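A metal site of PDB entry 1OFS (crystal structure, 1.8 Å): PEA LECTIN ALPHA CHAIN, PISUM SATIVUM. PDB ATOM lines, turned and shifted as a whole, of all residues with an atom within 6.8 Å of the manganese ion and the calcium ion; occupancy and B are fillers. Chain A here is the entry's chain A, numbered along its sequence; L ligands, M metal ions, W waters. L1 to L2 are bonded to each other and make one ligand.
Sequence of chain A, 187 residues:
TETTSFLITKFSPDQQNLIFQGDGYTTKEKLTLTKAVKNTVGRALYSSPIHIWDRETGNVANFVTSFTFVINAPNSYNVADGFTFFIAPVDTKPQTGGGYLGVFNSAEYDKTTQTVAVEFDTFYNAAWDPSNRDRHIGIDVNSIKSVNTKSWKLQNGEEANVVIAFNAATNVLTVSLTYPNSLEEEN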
ATOM      1  N   ASP A  81      23.439 -19.462  10.677  1.00  0.00           N
ATOM      2  CA  ASP A  81      24.385 -19.769   9.610  1.00  0.00           C
ATOM      3  C   ASP A  81      24.880 -21.198   9.740  1.00  0.00           C
ATOM      4  O   ASP A  81      25.311 -21.813   8.775  1.00  0.00           O
ATOM      5  CB  ASP A  81      25.598 -18.850   9.667  1.00  0.00           C
ATOM      6  CG  ASP A  81      25.477 -17.702   8.706  1.00  0.00           C
ATOM      7  OD1 ASP A  81      25.186 -16.582   9.170  1.00  0.00           O
ATOM      8  OD2 ASP A  81      25.631 -17.842   7.481  1.00  0.00           O
ATOM      9  N   GLY A  98      28.916 -14.867  11.132  1.00  0.00           N
ATOM     10  CA  GLY A  98      28.117 -15.070   9.944  1.00  0.00           C
ATOM     11  C   GLY A  98      28.498 -16.370   9.257  1.00  0.00           C
ATOM     12  O   GLY A  98      28.679 -17.417   9.899  1.00  0.00           O
ATOM     13  N   GLY A  99      28.656 -16.299   7.935  1.00  0.00           N
ATOM     14  CA  GLY A  99      29.002 -17.455   7.126  1.00  0.00           C
ATOM     15  C   GLY A  99      30.343 -18.097   7.439  1.00  0.00           C
ATOM     16  O   GLY A  99      30.621 -19.184   6.943  1.00  0.00           O
ATOM     17  N   TYR A 100      31.176 -17.420   8.231  1.00  0.00           N
ATOM     18  CA  TYR A 100      32.480 -17.962   8.615  1.00  0.00           C
ATOM     19  C   TYR A 100      32.417 -18.865   9.849  1.00  0.00           C
ATOM     20  O   TYR A 100      33.424 -19.410  10.283  1.00  0.00           O
ATOM     21  CB  TYR A 100      33.517 -16.850   8.781  1.00  0.00           C
ATOM     22  CG  TYR A 100      33.835 -16.155   7.470  1.00  0.00           C
ATOM     23  CD1 TYR A 100      33.165 -14.997   7.095  1.00  0.00           C
ATOM     24  CD2 TYR A 100      34.785 -16.677   6.593  1.00  0.00           C
ATOM     25  CE1 TYR A 100      33.445 -14.360   5.894  1.00  0.00           C
ATOM     26  CE2 TYR A 100      35.067 -16.055   5.383  1.00  0.00           C
ATOM     27  CZ  TYR A 100      34.399 -14.888   5.048  1.00  0.00           C
ATOM     28  OH  TYR A 100      34.658 -14.251   3.854  1.00  0.00           O
ATOM     29  N   LEU A 101      31.216 -18.997  10.419  1.00  0.00           N
ATOM     30  CA  LEU A 101      30.932 -19.892  11.556  1.00  0.00           C
ATOM     31  C   LEU A 101      31.762 -19.729  12.823  1.00  0.00           C
ATOM     32  O   LEU A 101      31.805 -20.637  13.664  1.00  0.00           O
ATOM     33  CB  LEU A 101      30.968 -21.361  11.075  1.00  0.00           C
ATOM     34  CG  LEU A 101      30.037 -21.619   9.877  1.00  0.00           C
ATOM     35  CD1 LEU A 101      30.171 -23.039   9.313  1.00  0.00           C
ATOM     36  CD2 LEU A 101      28.602 -21.364  10.322  1.00  0.00           C
ATOM     37  N   GLU A 119      31.570 -28.800   9.872  1.00  0.00           N
ATOM     38  CA  GLU A 119      30.454 -27.861   9.820  1.00  0.00           C
ATOM     39  C   GLU A 119      29.118 -28.461   9.416  1.00  0.00           C
ATOM     40  O   GLU A 119      29.057 -29.435   8.667  1.00  0.00           O
ATOM     41  CB  GLU A 119      30.774 -26.710   8.842  1.00  0.00           C
ATOM     42  CG  GLU A 119      30.919 -27.158   7.383  1.00  0.00           C
ATOM     43  CD  GLU A 119      30.992 -25.984   6.419  1.00  0.00           C
ATOM     44  OE1 GLU A 119      30.256 -25.980   5.420  1.00  0.00           O
ATOM     45  OE2 GLU A 119      31.790 -25.048   6.670  1.00  0.00           O
ATOM     46  N   ASP A 121      26.360 -26.598   7.965  1.00  0.00           N
ATOM     47  CA  ASP A 121      26.098 -25.332   7.289  1.00  0.00           C
ATOM     48  C   ASP A 121      24.676 -25.205   6.775  1.00  0.00           C
ATOM     49  O   ASP A 121      24.285 -25.924   5.868  1.00  0.00           O
ATOM     50  CB  ASP A 121      27.115 -25.246   6.128  1.00  0.00           C
ATOM     51  CG  ASP A 121      27.254 -23.862   5.570  1.00  0.00           C
ATOM     52  OD1 ASP A 121      26.340 -23.042   5.778  1.00  0.00           O
ATOM     53  OD2 ASP A 121      28.243 -23.501   4.864  1.00  0.00           O
ATOM     54  N   THR A 122      23.920 -24.255   7.312  1.00  0.00           N
ATOM     55  CA  THR A 122      22.518 -24.080   6.943  1.00  0.00           C
ATOM     56  C   THR A 122      22.212 -22.970   5.943  1.00  0.00           C
ATOM     57  O   THR A 122      21.058 -22.772   5.567  1.00  0.00           O
ATOM     58  CB  THR A 122      21.672 -23.794   8.204  1.00  0.00           C
ATOM     59  OG1 THR A 122      22.234 -22.683   8.907  1.00  0.00           O
ATOM     60  CG2 THR A 122      21.735 -24.955   9.193  1.00  0.00           C
ATOM     61  N   PHE A 123      23.232 -22.218   5.540  1.00  0.00           N
ATOM     62  CA  PHE A 123      23.016 -21.096   4.617  1.00  0.00           C
ATOM     63  C   PHE A 123      24.007 -21.087   3.461  1.00  0.00           C
ATOM     64  O   PHE A 123      25.214 -21.207   3.647  1.00  0.00           O
ATOM     65  CB  PHE A 123      23.086 -19.773   5.398  1.00  0.00           C
ATOM     66  CG  PHE A 123      22.908 -18.553   4.538  1.00  0.00           C
ATOM     67  CD1 PHE A 123      21.647 -18.032   4.290  1.00  0.00           C
ATOM     68  CD2 PHE A 123      24.006 -17.918   3.970  1.00  0.00           C
ATOM     69  CE1 PHE A 123      21.485 -16.904   3.499  1.00  0.00           C
ATOM     70  CE2 PHE A 123      23.855 -16.793   3.186  1.00  0.00           C
ATOM     71  CZ  PHE A 123      22.592 -16.280   2.951  1.00  0.00           C
ATOM     72  N   TYR A 124      23.492 -20.907   2.247  1.00  0.00           N
ATOM     73  CA  TYR A 124      24.344 -20.889   1.054  1.00  0.00           C
ATOM     74  C   TYR A 124      25.107 -19.580   0.877  1.00  0.00           C
ATOM     75  O   TYR A 124      24.507 -18.531   0.599  1.00  0.00           O
ATOM     76  CB  TYR A 124      23.516 -21.186  -0.209  1.00  0.00           C
ATOM     77  CG  TYR A 124      24.239 -20.916  -1.520  1.00  0.00           C
ATOM     78  CD1 TYR A 124      25.365 -21.652  -1.879  1.00  0.00           C
ATOM     79  CD2 TYR A 124      23.788 -19.947  -2.392  1.00  0.00           C
ATOM     80  CE1 TYR A 124      26.020 -21.406  -3.085  1.00  0.00           C
ATOM     81  CE2 TYR A 124      24.434 -19.696  -3.597  1.00  0.00           C
ATOM     82  CZ  TYR A 124      25.544 -20.431  -3.930  1.00  0.00           C
ATOM     83  OH  TYR A 124      26.190 -20.180  -5.135  1.00  0.00           O
ATOM     84  N   ASN A 125      26.418 -19.640   1.038  1.00  0.00           N
ATOM     85  CA  ASN A 125      27.296 -18.501   0.828  1.00  0.00           C
ATOM     86  C   ASN A 125      27.874 -18.744  -0.563  1.00  0.00           C
ATOM     87  O   ASN A 125      28.748 -19.585  -0.748  1.00  0.00           O
ATOM     88  CB  ASN A 125      28.404 -18.442   1.886  1.00  0.00           C
ATOM     89  CG  ASN A 125      27.884 -18.125   3.273  1.00  0.00           C
ATOM     90  OD1 ASN A 125      27.669 -19.014   4.088  1.00  0.00           O
ATOM     91  ND2 ASN A 125      27.682 -16.833   3.548  1.00  0.00           N
ATOM     92  N   TRP A 128      31.682 -19.488  -1.733  1.00  0.00           N
ATOM     93  CA  TRP A 128      32.411 -20.716  -1.501  1.00  0.00           C
ATOM     94  C   TRP A 128      31.616 -21.999  -1.266  1.00  0.00           C
ATOM     95  O   TRP A 128      32.165 -23.087  -1.397  1.00  0.00           O
ATOM     96  CB  TRP A 128      33.378 -20.513  -0.327  1.00  0.00           C
ATOM     97  CG  TRP A 128      32.664 -20.193   0.946  1.00  0.00           C
ATOM     98  CD1 TRP A 128      31.964 -21.064   1.735  1.00  0.00           C
ATOM     99  CD2 TRP A 128      32.575 -18.915   1.567  1.00  0.00           C
ATOM    100  NE1 TRP A 128      31.438 -20.392   2.813  1.00  0.00           N
ATOM    101  CE2 TRP A 128      31.796 -19.079   2.745  1.00  0.00           C
ATOM    102  CE3 TRP A 128      33.079 -17.642   1.266  1.00  0.00           C
ATOM    103  CZ2 TRP A 128      31.514 -18.019   3.599  1.00  0.00           C
ATOM    104  CZ3 TRP A 128      32.786 -16.601   2.114  1.00  0.00           C
ATOM    105  CH2 TRP A 128      32.015 -16.786   3.272  1.00  0.00           C
ATOM    106  N   ASP A 129      30.333 -21.884  -0.899  1.00  0.00           N
ATOM    107  CA  ASP A 129      29.535 -23.076  -0.621  1.00  0.00           C
ATOM    108  C   ASP A 129      29.161 -23.855  -1.891  1.00  0.00           C
ATOM    109  O   ASP A 129      29.220 -23.298  -2.991  1.00  0.00           O
ATOM    110  CB  ASP A 129      28.275 -22.714   0.181  1.00  0.00           C
ATOM    111  CG  ASP A 129      28.561 -22.507   1.664  1.00  0.00           C
ATOM    112  OD1 ASP A 129      29.495 -23.167   2.183  1.00  0.00           O
ATOM    113  OD2 ASP A 129      27.924 -21.715   2.374  1.00  0.00           O
ATOM    114  N   PRO A 130      28.817 -25.131  -1.738  1.00  0.00           N
ATOM    115  CA  PRO A 130      28.453 -25.964  -2.890  1.00  0.00           C
ATOM    116  C   PRO A 130      27.386 -25.282  -3.760  1.00  0.00           C
ATOM    117  O   PRO A 130      26.383 -24.799  -3.250  1.00  0.00           O
ATOM    118  CB  PRO A 130      27.912 -27.238  -2.235  1.00  0.00           C
ATOM    119  CG  PRO A 130      28.661 -27.301  -0.940  1.00  0.00           C
ATOM    120  CD  PRO A 130      28.761 -25.873  -0.471  1.00  0.00           C
ATOM    121  N   HIS A 136      24.464 -28.299   4.064  1.00  0.00           N
ATOM    122  CA  HIS A 136      25.400 -29.397   3.954  1.00  0.00           C
ATOM    123  C   HIS A 136      26.324 -29.563   5.140  1.00  0.00           C
ATOM    124  O   HIS A 136      26.527 -28.642   5.929  1.00  0.00           O
ATOM    125  CB  HIS A 136      26.309 -29.117   2.748  1.00  0.00           C
ATOM    126  CG  HIS A 136      26.911 -27.736   2.763  1.00  0.00           C
ATOM    127  ND1 HIS A 136      26.232 -26.628   2.302  1.00  0.00           N
ATOM    128  CD2 HIS A 136      28.112 -27.291   3.210  1.00  0.00           C
ATOM    129  CE1 HIS A 136      26.983 -25.560   2.457  1.00  0.00           C
ATOM    130  NE2 HIS A 136      28.136 -25.929   3.009  1.00  0.00           N
ATOM    131  N   ILE A 137      26.870 -30.769   5.262  1.00  0.00           N
ATOM    132  CA  ILE A 137      27.854 -31.081   6.270  1.00  0.00           C
ATOM    133  C   ILE A 137      29.170 -30.917   5.530  1.00  0.00           C
ATOM    134  O   ILE A 137      29.256 -31.233   4.333  1.00  0.00           O
ATOM    135  CB  ILE A 137      27.710 -32.521   6.774  1.00  0.00           C
ATOM    136  CG1 ILE A 137      26.326 -32.725   7.402  1.00  0.00           C
ATOM    137  CG2 ILE A 137      28.816 -32.848   7.803  1.00  0.00           C
ATOM    138  CD1 ILE A 137      26.009 -34.178   7.714  1.00  0.00           C
ATOM    139  N   GLY A 138      30.198 -30.412   6.194  1.00  0.00           N
ATOM    140  CA  GLY A 138      31.478 -30.238   5.525  1.00  0.00           C
ATOM    141  C   GLY A 138      32.661 -30.426   6.434  1.00  0.00           C
ATOM    142  O   GLY A 138      32.539 -30.334   7.655  1.00  0.00           O
ATOM    143  N   ASP A 140      36.234 -28.821   7.138  1.00  0.00           N
ATOM    144  CA  ASP A 140      36.989 -27.592   6.888  1.00  0.00           C
ATOM    145  C   ASP A 140      38.403 -27.670   7.409  1.00  0.00           C
ATOM    146  O   ASP A 140      38.620 -28.019   8.578  1.00  0.00           O
ATOM    147  CB  ASP A 140      36.302 -26.411   7.588  1.00  0.00           C
ATOM    148  CG  ASP A 140      34.875 -26.202   7.129  1.00  0.00           C
ATOM    149  OD1 ASP A 140      34.470 -26.837   6.122  1.00  0.00           O
ATOM    150  OD2 ASP A 140      34.097 -25.402   7.699  1.00  0.00           O
ATOM    151  N   ILE A 144      37.067 -21.710   5.278  1.00  0.00           N
ATOM    152  CA  ILE A 144      35.618 -21.924   5.310  1.00  0.00           C
ATOM    153  C   ILE A 144      35.136 -22.681   4.067  1.00  0.00           C
ATOM    154  O   ILE A 144      34.013 -23.191   4.023  1.00  0.00           O
ATOM    155  CB  ILE A 144      34.886 -20.586   5.494  1.00  0.00           C
ATOM    156  CG1 ILE A 144      33.419 -20.809   5.886  1.00  0.00           C
ATOM    157  CG2 ILE A 144      35.006 -19.737   4.230  1.00  0.00           C
ATOM    158  CD1 ILE A 144      33.236 -21.400   7.274  1.00  0.00           C
ATOM    159  N   LYS A 145      35.991 -22.758   3.051  1.00  0.00           N
ATOM    160  CA  LYS A 145      35.676 -23.514   1.846  1.00  0.00           C
ATOM    161  C   LYS A 145      36.072 -24.954   2.119  1.00  0.00           C
ATOM    162  O   LYS A 145      37.263 -25.310   2.033  1.00  0.00           O
ATOM    163  CB  LYS A 145      36.443 -22.970   0.638  1.00  0.00           C
ATOM    164  CG  LYS A 145      36.055 -23.648  -0.660  1.00  0.00           C
ATOM    165  CD  LYS A 145      36.962 -23.233  -1.818  1.00  0.00           C
ATOM    166  CE  LYS A 145      36.583 -23.946  -3.105  1.00  0.00           C
ATOM    167  NZ  LYS A 145      35.159 -24.400  -3.095  1.00  0.00           N
ATOM    168  N   SER A 146      35.083 -25.787   2.429  1.00  0.00           N
ATOM    169  CA  SER A 146      35.330 -27.191   2.770  1.00  0.00           C
ATOM    170  C   SER A 146      36.109 -28.018   1.745  1.00  0.00           C
ATOM    171  O   SER A 146      36.007 -27.785   0.537  1.00  0.00           O
ATOM    172  CB  SER A 146      34.001 -27.900   3.065  1.00  0.00           C
ATOM    173  OG  SER A 146      33.101 -27.075   3.800  1.00  0.00           O
ATOM    174  N   THR A 149      32.135 -32.057   1.152  1.00  0.00           N
ATOM    175  CA  THR A 149      30.812 -31.774   1.688  1.00  0.00           C
ATOM    176  C   THR A 149      29.833 -32.882   1.359  1.00  0.00           C
ATOM    177  O   THR A 149      30.111 -33.763   0.549  1.00  0.00           O
ATOM    178  CB  THR A 149      30.234 -30.457   1.113  1.00  0.00           C
ATOM    179  OG1 THR A 149      30.296 -30.505  -0.326  1.00  0.00           O
ATOM    180  CG2 THR A 149      31.091 -29.249   1.495  1.00  0.00           C
HETATM  181  C1  LIG L   1      24.969 -11.939   5.757  1.00  0.00           C
HETATM  182  C2  LIG L   1      26.375 -12.230   6.304  1.00  0.00           C
HETATM  183  C3  LIG L   1      26.834 -13.649   5.880  1.00  0.00           C
HETATM  184  C4  LIG L   1      25.814 -14.679   6.388  1.00  0.00           C
HETATM  185  C5  LIG L   1      24.406 -14.320   5.834  1.00  0.00           C
HETATM  186  C6  LIG L   1      23.263 -15.199   6.326  1.00  0.00           C
HETATM  187  O1  LIG L   1      27.275 -11.282   5.796  1.00  0.00           O
HETATM  188  O2  LIG L   1      28.101 -13.900   6.482  1.00  0.00           O
HETATM  189  O3  LIG L   1      26.175 -15.976   5.914  1.00  0.00           O
HETATM  190  O4  LIG L   1      24.062 -12.950   6.273  1.00  0.00           O
HETATM  191  O5  LIG L   1      23.238 -15.145   7.765  1.00  0.00           O
HETATM  192  C1  LG2 L   2      24.843  -9.576   3.952  1.00  0.00           C
HETATM  193  C2  LG2 L   2      24.237 -10.946   3.686  1.00  0.00           C
HETATM  194  C3  LG2 L   2      24.167 -11.254   2.177  1.00  0.00           C
HETATM  195  C4  LG2 L   2      23.166 -12.374   2.189  1.00  0.00           C
HETATM  196  C5  LG2 L   2      22.108 -11.718   3.101  1.00  0.00           C
HETATM  197  C6  LG2 L   2      21.190 -12.723   3.765  1.00  0.00           C
HETATM  198  O1  LG2 L   2      23.984  -8.549   3.423  1.00  0.00           O
HETATM  199  O2  LG2 L   2      25.008 -11.958   4.352  1.00  0.00           O
HETATM  200  O3  LG2 L   2      25.426 -11.711   1.688  1.00  0.00           O
HETATM  201  O4  LG2 L   2      22.630 -12.587   0.878  1.00  0.00           O
HETATM  202  O5  LG2 L   2      22.879 -10.986   4.112  1.00  0.00           O
HETATM  203  O6  LG2 L   2      20.055 -12.063   4.260  1.00  0.00           O
HETATM  204 MN    MN M   1      29.755 -24.542   3.830  1.00  0.00          MN
HETATM  205 CA    CA M   2      27.347 -21.257   4.595  1.00  0.00          CA
HETATM  206  O   HOH W   1      26.670 -20.259   6.647  1.00  0.00           O
HETATM  207  O   HOH W   2      29.701 -21.019   5.232  1.00  0.00           O
HETATM  208  O   HOH W   3      31.380 -23.309   4.814  1.00  0.00           O
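Within 4 Å of the calcium ion: Asp 121, Phe 123, Asn 125 and Asp 129. The nearest printed residue that does not touch the calcium ion is Tyr 124 (4.5 Å).
The calcium ion is bound by OD1 of Asn 125 (2.3 Å). The calcium ion is bound by O of Phe 123 (2.3 Å). The calcium ion is bound by OD2 of Asp 129, 2.3 Å away. OD1 of Asp 121 is bound to the calcium ion, at 2.4 Å. The calcium ion is bound by water W1 (2.4 Å). The calcium ion is bound by the side-chain carboxylate (OD2) of Asp 121, at 2.4 Å. The calcium ion is bound by water W2 (2.5 Å).
The side-chain carboxylate (OD2) of Asp 121 binds the manganese ion (2.1 Å). The side-chain carboxylate (OD1) of Asp 129 is bound to the manganese ion, at 2.2 Å. The side-chain carboxylate (OE1) of Glu 119 binds the manganese ion (2.2 Å). The manganese ion is bound by water W3. NE2 of His 136 binds the manganese ion. The manganese ion has five donor atoms within binding distance.
Four residues have an atom within 4 Å of the manganese ion: Glu 119, Asp 121, Asp 129 and His 136. Along chain A the residues within 4 Å of the manganese ion span positions 119 to 136.
ND2 of Asn 125 is in hydrogen-bond range of O3 of LIG L1 (2.9 Å). O2 of LIG L1 sits at hydrogen-bond distance from N of Gly 99, 2.9 Å away. OD2 of Asp 81 lies within hydrogen-bond range of O3 of LIG L1, at 2.5 Å.
The side-chain carboxylate of Asp 129 lies close to the indole nitrogen of Trp 128, at 3.4 Å. The side-chain carboxylate (OE1) of Glu 119 sits close to the side-chain hydroxyl (OG) of Ser 146 (3.5 Å). The side-chain carboxylate (OE2) of Glu 119 lies close to the side-chain carboxylate (OD2) of Asp 140, at 2.6 Å. The backbone NH (N) of Glu 119 is in hydrogen-bond range of the backbone carbonyl oxygen (O) of Gly 138, at 2.9 Å.
Water W3 bridges the side-chain carboxylate (OE2) of Glu 119 and the backbone carbonyl oxygen (O) of Ile 144. Water W2 bridges O of Gly 99 and NE1 of Trp 128.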
